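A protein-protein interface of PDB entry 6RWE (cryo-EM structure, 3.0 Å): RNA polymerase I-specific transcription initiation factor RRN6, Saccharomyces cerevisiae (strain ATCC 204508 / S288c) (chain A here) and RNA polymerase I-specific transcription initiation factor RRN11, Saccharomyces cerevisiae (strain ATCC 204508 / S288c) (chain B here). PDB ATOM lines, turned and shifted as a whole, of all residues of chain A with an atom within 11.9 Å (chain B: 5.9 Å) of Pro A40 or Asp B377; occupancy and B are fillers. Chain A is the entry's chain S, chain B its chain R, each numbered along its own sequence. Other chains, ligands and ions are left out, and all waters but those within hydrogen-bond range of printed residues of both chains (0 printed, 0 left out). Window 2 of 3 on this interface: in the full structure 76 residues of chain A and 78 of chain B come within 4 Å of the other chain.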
ATOM      1  N   LYS A  36       0.678 -13.054  38.122  1.00  0.00           N
ATOM      2  CA  LYS A  36       1.579 -13.973  37.438  1.00  0.00           C
ATOM      3  C   LYS A  36       1.893 -13.372  36.082  1.00  0.00           C
ATOM      4  O   LYS A  36       0.993 -12.888  35.398  1.00  0.00           O
ATOM      5  CB  LYS A  36       0.981 -15.379  37.260  1.00  0.00           C
ATOM      6  CG  LYS A  36       1.864 -16.322  36.434  1.00  0.00           C
ATOM      7  CD  LYS A  36       1.456 -17.783  36.493  1.00  0.00           C
ATOM      8  CE  LYS A  36       0.238 -18.079  35.682  1.00  0.00           C
ATOM      9  NZ  LYS A  36       0.062 -19.547  35.664  1.00  0.00           N
ATOM     10  N   GLN A  37       3.164 -13.391  35.698  1.00  0.00           N
ATOM     11  CA  GLN A  37       3.515 -12.932  34.364  1.00  0.00           C
ATOM     12  C   GLN A  37       3.405 -14.004  33.299  1.00  0.00           C
ATOM     13  O   GLN A  37       3.195 -13.660  32.129  1.00  0.00           O
ATOM     14  CB  GLN A  37       4.939 -12.391  34.333  1.00  0.00           C
ATOM     15  CG  GLN A  37       5.092 -11.104  35.040  1.00  0.00           C
ATOM     16  CD  GLN A  37       4.165 -10.078  34.496  1.00  0.00           C
ATOM     17  OE1 GLN A  37       3.234  -9.674  35.165  1.00  0.00           O
ATOM     18  NE2 GLN A  37       4.396  -9.662  33.263  1.00  0.00           N
ATOM     19  N   GLU A  38       3.543 -15.276  33.681  1.00  0.00           N
ATOM     20  CA  GLU A  38       3.837 -16.375  32.759  1.00  0.00           C
ATOM     21  C   GLU A  38       5.099 -16.043  31.955  1.00  0.00           C
ATOM     22  O   GLU A  38       5.061 -15.604  30.808  1.00  0.00           O
ATOM     23  CB  GLU A  38       2.626 -16.744  31.883  1.00  0.00           C
ATOM     24  CG  GLU A  38       2.838 -17.870  30.865  1.00  0.00           C
ATOM     25  CD  GLU A  38       3.174 -19.203  31.481  1.00  0.00           C
ATOM     26  OE1 GLU A  38       2.787 -19.457  32.637  1.00  0.00           O
ATOM     27  OE2 GLU A  38       3.827 -20.014  30.798  1.00  0.00           O
ATOM     28  N   LYS A  39       6.213 -16.099  32.675  1.00  0.00           N
ATOM     29  CA  LYS A  39       7.544 -16.002  32.096  1.00  0.00           C
ATOM     30  C   LYS A  39       8.063 -17.387  31.728  1.00  0.00           C
ATOM     31  O   LYS A  39       8.575 -18.095  32.600  1.00  0.00           O
ATOM     32  CB  LYS A  39       8.510 -15.358  33.088  1.00  0.00           C
ATOM     33  CG  LYS A  39       8.181 -13.949  33.501  1.00  0.00           C
ATOM     34  CD  LYS A  39       8.399 -12.981  32.357  1.00  0.00           C
ATOM     35  CE  LYS A  39       8.253 -11.541  32.817  1.00  0.00           C
ATOM     36  NZ  LYS A  39       9.387 -11.109  33.685  1.00  0.00           N
ATOM     37  N   PRO A  40       7.986 -17.806  30.462  1.00  0.00           N
ATOM     38  CA  PRO A  40       8.440 -19.160  30.114  1.00  0.00           C
ATOM     39  C   PRO A  40       9.960 -19.278  30.088  1.00  0.00           C
ATOM     40  O   PRO A  40      10.580 -19.258  29.020  1.00  0.00           O
ATOM     41  CB  PRO A  40       7.826 -19.384  28.729  1.00  0.00           C
ATOM     42  CG  PRO A  40       7.716 -18.019  28.152  1.00  0.00           C
ATOM     43  CD  PRO A  40       7.459 -17.085  29.293  1.00  0.00           C
ATOM     44  N   GLN A  41      10.572 -19.425  31.267  1.00  0.00           N
ATOM     45  CA  GLN A  41      12.023 -19.352  31.381  1.00  0.00           C
ATOM     46  C   GLN A  41      12.634 -20.490  32.194  1.00  0.00           C
ATOM     47  O   GLN A  41      13.825 -20.414  32.524  1.00  0.00           O
ATOM     48  CB  GLN A  41      12.430 -18.007  31.993  1.00  0.00           C
ATOM     49  CG  GLN A  41      11.982 -17.827  33.436  1.00  0.00           C
ATOM     50  CD  GLN A  41      12.351 -16.469  34.000  1.00  0.00           C
ATOM     51  OE1 GLN A  41      12.925 -15.629  33.307  1.00  0.00           O
ATOM     52  NE2 GLN A  41      12.042 -16.255  35.275  1.00  0.00           N
ATOM     53  N   TRP A  42      11.851 -21.522  32.541  1.00  0.00           N
ATOM     54  CA  TRP A  42      12.267 -22.701  33.317  1.00  0.00           C
ATOM     55  C   TRP A  42      12.818 -22.350  34.700  1.00  0.00           C
ATOM     56  O   TRP A  42      13.544 -23.146  35.300  1.00  0.00           O
ATOM     57  CB  TRP A  42      13.298 -23.553  32.559  1.00  0.00           C
ATOM     58  CG  TRP A  42      12.763 -24.247  31.356  1.00  0.00           C
ATOM     59  CD1 TRP A  42      12.834 -23.820  30.062  1.00  0.00           C
ATOM     60  CD2 TRP A  42      12.088 -25.509  31.326  1.00  0.00           C
ATOM     61  NE1 TRP A  42      12.235 -24.733  29.229  1.00  0.00           N
ATOM     62  CE2 TRP A  42      11.771 -25.780  29.981  1.00  0.00           C
ATOM     63  CE3 TRP A  42      11.716 -26.432  32.308  1.00  0.00           C
ATOM     64  CZ2 TRP A  42      11.097 -26.937  29.593  1.00  0.00           C
ATOM     65  CZ3 TRP A  42      11.050 -27.579  31.921  1.00  0.00           C
ATOM     66  CH2 TRP A  42      10.746 -27.822  30.574  1.00  0.00           C
ATOM     67  N   LEU A  43      12.471 -21.181  35.229  1.00  0.00           N
ATOM     68  CA  LEU A  43      13.096 -20.624  36.425  1.00  0.00           C
ATOM     69  C   LEU A  43      11.988 -20.104  37.343  1.00  0.00           C
ATOM     70  O   LEU A  43      11.914 -18.915  37.648  1.00  0.00           O
ATOM     71  CB  LEU A  43      14.132 -19.559  36.033  1.00  0.00           C
ATOM     72  CG  LEU A  43      15.283 -19.155  36.974  1.00  0.00           C
ATOM     73  CD1 LEU A  43      16.524 -18.851  36.142  1.00  0.00           C
ATOM     74  CD2 LEU A  43      14.983 -17.956  37.870  1.00  0.00           C
ATOM     75  N   ARG A  44      11.052 -21.013  37.694  1.00  0.00           N
ATOM     76  CA  ARG A  44       9.802 -20.751  38.405  1.00  0.00           C
ATOM     77  C   ARG A  44       8.940 -19.799  37.587  1.00  0.00           C
ATOM     78  O   ARG A  44       8.877 -18.601  37.893  1.00  0.00           O
ATOM     79  CB  ARG A  44      10.033 -20.195  39.817  1.00  0.00           C
ATOM     80  CG  ARG A  44      10.639 -21.192  40.780  1.00  0.00           C
ATOM     81  CD  ARG A  44      10.636 -20.656  42.199  1.00  0.00           C
ATOM     82  NE  ARG A  44      11.488 -19.479  42.340  1.00  0.00           N
ATOM     83  CZ  ARG A  44      12.783 -19.525  42.638  1.00  0.00           C
ATOM     84  NH1 ARG A  44      13.482 -18.404  42.745  1.00  0.00           N
ATOM     85  NH2 ARG A  44      13.380 -20.694  42.829  1.00  0.00           N
ATOM     86  N   PRO A  45       8.265 -20.292  36.521  1.00  0.00           N
ATOM     87  CA  PRO A  45       7.623 -19.402  35.537  1.00  0.00           C
ATOM     88  C   PRO A  45       6.416 -18.624  36.042  1.00  0.00           C
ATOM     89  O   PRO A  45       5.353 -18.637  35.417  1.00  0.00           O
ATOM     90  CB  PRO A  45       7.191 -20.379  34.437  1.00  0.00           C
ATOM     91  CG  PRO A  45       6.954 -21.653  35.156  1.00  0.00           C
ATOM     92  CD  PRO A  45       7.983 -21.711  36.246  1.00  0.00           C
ATOM     93  N   VAL A  46       6.592 -17.918  37.152  1.00  0.00           N
ATOM     94  CA  VAL A  46       5.550 -17.183  37.845  1.00  0.00           C
ATOM     95  C   VAL A  46       6.258 -16.232  38.802  1.00  0.00           C
ATOM     96  O   VAL A  46       7.254 -16.602  39.430  1.00  0.00           O
ATOM     97  CB  VAL A  46       4.580 -18.157  38.550  1.00  0.00           C
ATOM     98  CG1 VAL A  46       5.335 -19.197  39.375  1.00  0.00           C
ATOM     99  CG2 VAL A  46       3.621 -17.424  39.448  1.00  0.00           C
ATOM    100  N   ASP A  47       5.792 -14.995  38.899  1.00  0.00           N
ATOM    101  CA  ASP A  47       6.400 -14.086  39.858  1.00  0.00           C
ATOM    102  C   ASP A  47       5.362 -13.633  40.876  1.00  0.00           C
ATOM    103  O   ASP A  47       5.100 -12.436  41.023  1.00  0.00           O
ATOM    104  CB  ASP A  47       7.108 -12.915  39.172  1.00  0.00           C
ATOM    105  CG  ASP A  47       6.213 -12.130  38.262  1.00  0.00           C
ATOM    106  OD1 ASP A  47       5.072 -12.565  38.007  1.00  0.00           O
ATOM    107  OD2 ASP A  47       6.648 -11.040  37.851  1.00  0.00           O
ATOM    108  N   HIS B 372      -5.481 -17.655  28.040  1.00  0.00           N
ATOM    109  CA  HIS B 372      -5.156 -17.921  26.645  1.00  0.00           C
ATOM    110  C   HIS B 372      -3.671 -17.796  26.380  1.00  0.00           C
ATOM    111  O   HIS B 372      -3.145 -18.494  25.509  1.00  0.00           O
ATOM    112  CB  HIS B 372      -5.914 -16.975  25.722  1.00  0.00           C
ATOM    113  CG  HIS B 372      -7.388 -17.195  25.721  1.00  0.00           C
ATOM    114  ND1 HIS B 372      -7.970 -18.306  25.154  1.00  0.00           N
ATOM    115  CD2 HIS B 372      -8.403 -16.440  26.200  1.00  0.00           C
ATOM    116  CE1 HIS B 372      -9.280 -18.233  25.296  1.00  0.00           C
ATOM    117  NE2 HIS B 372      -9.569 -17.110  25.927  1.00  0.00           N
ATOM    118  N   LEU B 373      -2.992 -16.912  27.108  1.00  0.00           N
ATOM    119  CA  LEU B 373      -1.560 -16.738  26.919  1.00  0.00           C
ATOM    120  C   LEU B 373      -0.795 -17.977  27.344  1.00  0.00           C
ATOM    121  O   LEU B 373       0.260 -18.274  26.778  1.00  0.00           O
ATOM    122  CB  LEU B 373      -1.090 -15.513  27.696  1.00  0.00           C
ATOM    123  CG  LEU B 373       0.313 -14.962  27.460  1.00  0.00           C
ATOM    124  CD1 LEU B 373       0.245 -13.477  27.576  1.00  0.00           C
ATOM    125  CD2 LEU B 373       1.303 -15.473  28.478  1.00  0.00           C
ATOM    126  N   LEU B 374      -1.301 -18.703  28.330  1.00  0.00           N
ATOM    127  CA  LEU B 374      -0.700 -19.975  28.681  1.00  0.00           C
ATOM    128  C   LEU B 374      -1.042 -21.055  27.667  1.00  0.00           C
ATOM    129  O   LEU B 374      -0.253 -21.987  27.488  1.00  0.00           O
ATOM    130  CB  LEU B 374      -1.139 -20.369  30.091  1.00  0.00           C
ATOM    131  CG  LEU B 374      -0.515 -21.559  30.809  1.00  0.00           C
ATOM    132  CD1 LEU B 374      -0.414 -21.233  32.270  1.00  0.00           C
ATOM    133  CD2 LEU B 374      -1.370 -22.794  30.645  1.00  0.00           C
ATOM    134  N   LYS B 375      -2.185 -20.947  26.993  1.00  0.00           N
ATOM    135  CA  LYS B 375      -2.494 -21.871  25.908  1.00  0.00           C
ATOM    136  C   LYS B 375      -1.607 -21.618  24.701  1.00  0.00           C
ATOM    137  O   LYS B 375      -1.138 -22.561  24.058  1.00  0.00           O
ATOM    138  CB  LYS B 375      -3.961 -21.755  25.511  1.00  0.00           C
ATOM    139  CG  LYS B 375      -4.910 -22.323  26.512  1.00  0.00           C
ATOM    140  CD  LYS B 375      -4.757 -23.821  26.573  1.00  0.00           C
ATOM    141  CE  LYS B 375      -5.364 -24.498  25.371  1.00  0.00           C
ATOM    142  NZ  LYS B 375      -5.325 -25.978  25.541  1.00  0.00           N
ATOM    143  N   ALA B 376      -1.374 -20.345  24.380  1.00  0.00           N
ATOM    144  CA  ALA B 376      -0.524 -19.999  23.248  1.00  0.00           C
ATOM    145  C   ALA B 376       0.929 -20.359  23.522  1.00  0.00           C
ATOM    146  O   ALA B 376       1.717 -20.546  22.594  1.00  0.00           O
ATOM    147  CB  ALA B 376      -0.662 -18.514  22.925  1.00  0.00           C
ATOM    148  N   ASP B 377       1.305 -20.448  24.795  1.00  0.00           N
ATOM    149  CA  ASP B 377       2.648 -20.904  25.127  1.00  0.00           C
ATOM    150  C   ASP B 377       2.800 -22.392  24.852  1.00  0.00           C
ATOM    151  O   ASP B 377       3.786 -22.823  24.247  1.00  0.00           O
ATOM    152  CB  ASP B 377       2.951 -20.599  26.590  1.00  0.00           C
ATOM    153  CG  ASP B 377       4.423 -20.705  26.920  1.00  0.00           C
ATOM    154  OD1 ASP B 377       5.238 -20.953  26.010  1.00  0.00           O
ATOM    155  OD2 ASP B 377       4.766 -20.551  28.107  1.00  0.00           O
ATOM    156  N   THR B 378       1.829 -23.193  25.280  1.00  0.00           N
ATOM    157  CA  THR B 378       1.978 -24.641  25.219  1.00  0.00           C
ATOM    158  C   THR B 378       1.683 -25.175  23.821  1.00  0.00           C
ATOM    159  O   THR B 378       2.355 -26.101  23.355  1.00  0.00           O
ATOM    160  CB  THR B 378       1.070 -25.286  26.264  1.00  0.00           C
ATOM    161  OG1 THR B 378       1.388 -24.742  27.550  1.00  0.00           O
ATOM    162  CG2 THR B 378       1.272 -26.786  26.322  1.00  0.00           C
ATOM    163  N   LEU B 379       0.707 -24.591  23.127  1.00  0.00           N
ATOM    164  CA  LEU B 379       0.391 -25.050  21.778  1.00  0.00           C
ATOM    165  C   LEU B 379       1.476 -24.658  20.786  1.00  0.00           C
ATOM    166  O   LEU B 379       1.638 -25.307  19.748  1.00  0.00           O
ATOM    167  CB  LEU B 379      -0.959 -24.501  21.324  1.00  0.00           C
ATOM    168  CG  LEU B 379      -2.239 -25.288  21.614  1.00  0.00           C
ATOM    169  CD1 LEU B 379      -2.160 -26.660  20.971  1.00  0.00           C
ATOM    170  CD2 LEU B 379      -2.549 -25.404  23.088  1.00  0.00           C
ATOM    171  N   SER B 380       2.228 -23.602  21.080  1.00  0.00           N
ATOM    172  CA  SER B 380       3.319 -23.208  20.202  1.00  0.00           C
ATOM    173  C   SER B 380       4.624 -23.885  20.597  1.00  0.00           C
ATOM    174  O   SER B 380       5.592 -23.214  20.962  1.00  0.00           O
ATOM    175  CB  SER B 380       3.491 -21.694  20.202  1.00  0.00           C
ATOM    176  OG  SER B 380       4.572 -21.311  19.389  1.00  0.00           O
ATOM    177  N   ARG B 381       4.645 -25.212  20.550  1.00  0.00           N
ATOM    178  CA  ARG B 381       5.872 -25.995  20.612  1.00  0.00           C
ATOM    179  C   ARG B 381       6.117 -26.743  19.313  1.00  0.00           C
ATOM    180  O   ARG B 381       7.223 -26.678  18.756  1.00  0.00           O
ATOM    181  CB  ARG B 381       5.805 -26.990  21.780  1.00  0.00           C
ATOM    182  CG  ARG B 381       5.625 -26.359  23.141  1.00  0.00           C
ATOM    183  CD  ARG B 381       6.853 -25.599  23.592  1.00  0.00           C
ATOM    184  NE  ARG B 381       6.692 -25.095  24.951  1.00  0.00           N
ATOM    185  CZ  ARG B 381       7.582 -24.334  25.579  1.00  0.00           C
ATOM    186  NH1 ARG B 381       7.348 -23.920  26.816  1.00  0.00           N
ATOM    187  NH2 ARG B 381       8.705 -23.989  24.968  1.00  0.00           N
ATOM    188  N   GLN B 434       5.616 -10.919  24.524  1.00  0.00           N
ATOM    189  CA  GLN B 434       5.557 -12.361  24.688  1.00  0.00           C
ATOM    190  C   GLN B 434       4.772 -13.029  23.576  1.00  0.00           C
ATOM    191  O   GLN B 434       5.007 -14.202  23.276  1.00  0.00           O
ATOM    192  CB  GLN B 434       4.936 -12.714  26.037  1.00  0.00           C
ATOM    193  CG  GLN B 434       5.811 -12.351  27.204  1.00  0.00           C
ATOM    194  CD  GLN B 434       7.135 -13.069  27.145  1.00  0.00           C
ATOM    195  OE1 GLN B 434       8.181 -12.460  26.925  1.00  0.00           O
ATOM    196  NE2 GLN B 434       7.095 -14.382  27.316  1.00  0.00           N
ATOM    197  N   PHE B 438       5.828 -15.765  20.379  1.00  0.00           N
ATOM    198  CA  PHE B 438       5.045 -16.942  20.036  1.00  0.00           C
ATOM    199  C   PHE B 438       4.793 -17.033  18.541  1.00  0.00           C
ATOM    200  O   PHE B 438       4.503 -18.124  18.038  1.00  0.00           O
ATOM    201  CB  PHE B 438       3.712 -16.931  20.783  1.00  0.00           C
ATOM    202  CG  PHE B 438       3.836 -17.137  22.265  1.00  0.00           C
ATOM    203  CD1 PHE B 438       4.975 -17.700  22.817  1.00  0.00           C
ATOM    204  CD2 PHE B 438       2.809 -16.747  23.112  1.00  0.00           C
ATOM    205  CE1 PHE B 438       5.083 -17.879  24.183  1.00  0.00           C
ATOM    206  CE2 PHE B 438       2.911 -16.926  24.480  1.00  0.00           C
ATOM    207  CZ  PHE B 438       4.049 -17.490  25.014  1.00  0.00           C
ATOM    208  N   ARG B 441       8.062 -18.414  16.980  1.00  0.00           N
ATOM    209  CA  ARG B 441       8.000 -19.867  16.969  1.00  0.00           C
ATOM    210  C   ARG B 441       7.102 -20.380  15.856  1.00  0.00           C
ATOM    211  O   ARG B 441       7.189 -21.557  15.494  1.00  0.00           O
ATOM    212  CB  ARG B 441       7.479 -20.385  18.301  1.00  0.00           C
ATOM    213  CG  ARG B 441       8.330 -20.062  19.502  1.00  0.00           C
ATOM    214  CD  ARG B 441       7.676 -20.640  20.742  1.00  0.00           C
ATOM    215  NE  ARG B 441       8.372 -20.277  21.968  1.00  0.00           N
ATOM    216  CZ  ARG B 441       7.975 -20.645  23.178  1.00  0.00           C
ATOM    217  NH1 ARG B 441       8.663 -20.269  24.244  1.00  0.00           N
ATOM    218  NH2 ARG B 441       6.899 -21.402  23.319  1.00  0.00           N
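OD2 of Asp B377 sits close to OE2 of Glu A38, at 2.9 Å.
The backbone carbonyl oxygen (O) of Leu B374 lies within hydrogen-bond range of the side-chain hydroxyl (OG1) of Thr B378 (3.2 Å). The guanidinium group of Arg B381 lies within salt-bridge range of the side-chain carboxylate of Asp B377 (3.7 Å). The side-chain carboxylate (OD1) of Asp B377 lies within salt-bridge range of the guanidinium group (NH2) of Arg B441 (3.2 Å).
Among the printed residues, merely in contact across the chains: Pro A40 with Asp B377 (3.3 Å), Pro A40 with Gln B434 (3.4 Å), Glu A38 with Leu B374 (3.7 Å), Glu A38 with Leu B373 (3.7 Å) and Lys A36 with Leu B374 (3.8 Å).
Printed residues of chain B within 4 Å of Lys A36: Leu B374. Of the printed residues of chain B, Glu A38 touches Leu B373 (3.7 Å), Leu B374 (3.7 Å) and Asp B377 (2.9 Å). Pro A40 touches just these residues of chain B: Asp B377 (3.3 Å) and Gln B434 (3.4 Å). Leu B374 touches two residues of chain A. No residue of chain A comes within 4 Å of Ala B376. No residue of chain A comes within 4 Å of Leu B379. No residue of chain A comes within 4 Å of Ser B380. Of the printed residues of chain A, Gln B434 touches Pro A40 (3.4 Å). The nearest residue of chain B that does not touch Pro A40 is Arg B441 (4.6 Å). The nearest residue of chain A that does not touch Asp B377 is Lys A39 (5.8 Å). The nearest printed residue of chain B that does not touch Glu A38 is Gln B434 (4.2 Å).
Of the 12 printed residues of chain A, 3 touch a printed residue of chain B. Printed residues of chain A that touch a printed residue of chain B: Lys A36, Glu A38 and Pro A40. Hydrophobic or aromatic side chains of chain A within 4 Å of the printed part of chain B: Pro A40. Of the 13 printed residues of chain B, 4 touch a printed residue of chain A. Hydrophobic or aromatic side chains of chain B within 4 Å of the printed part of chain A: Leu B373 and Leu B374. Among the printed residues, 6 pairs touch across the chains.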
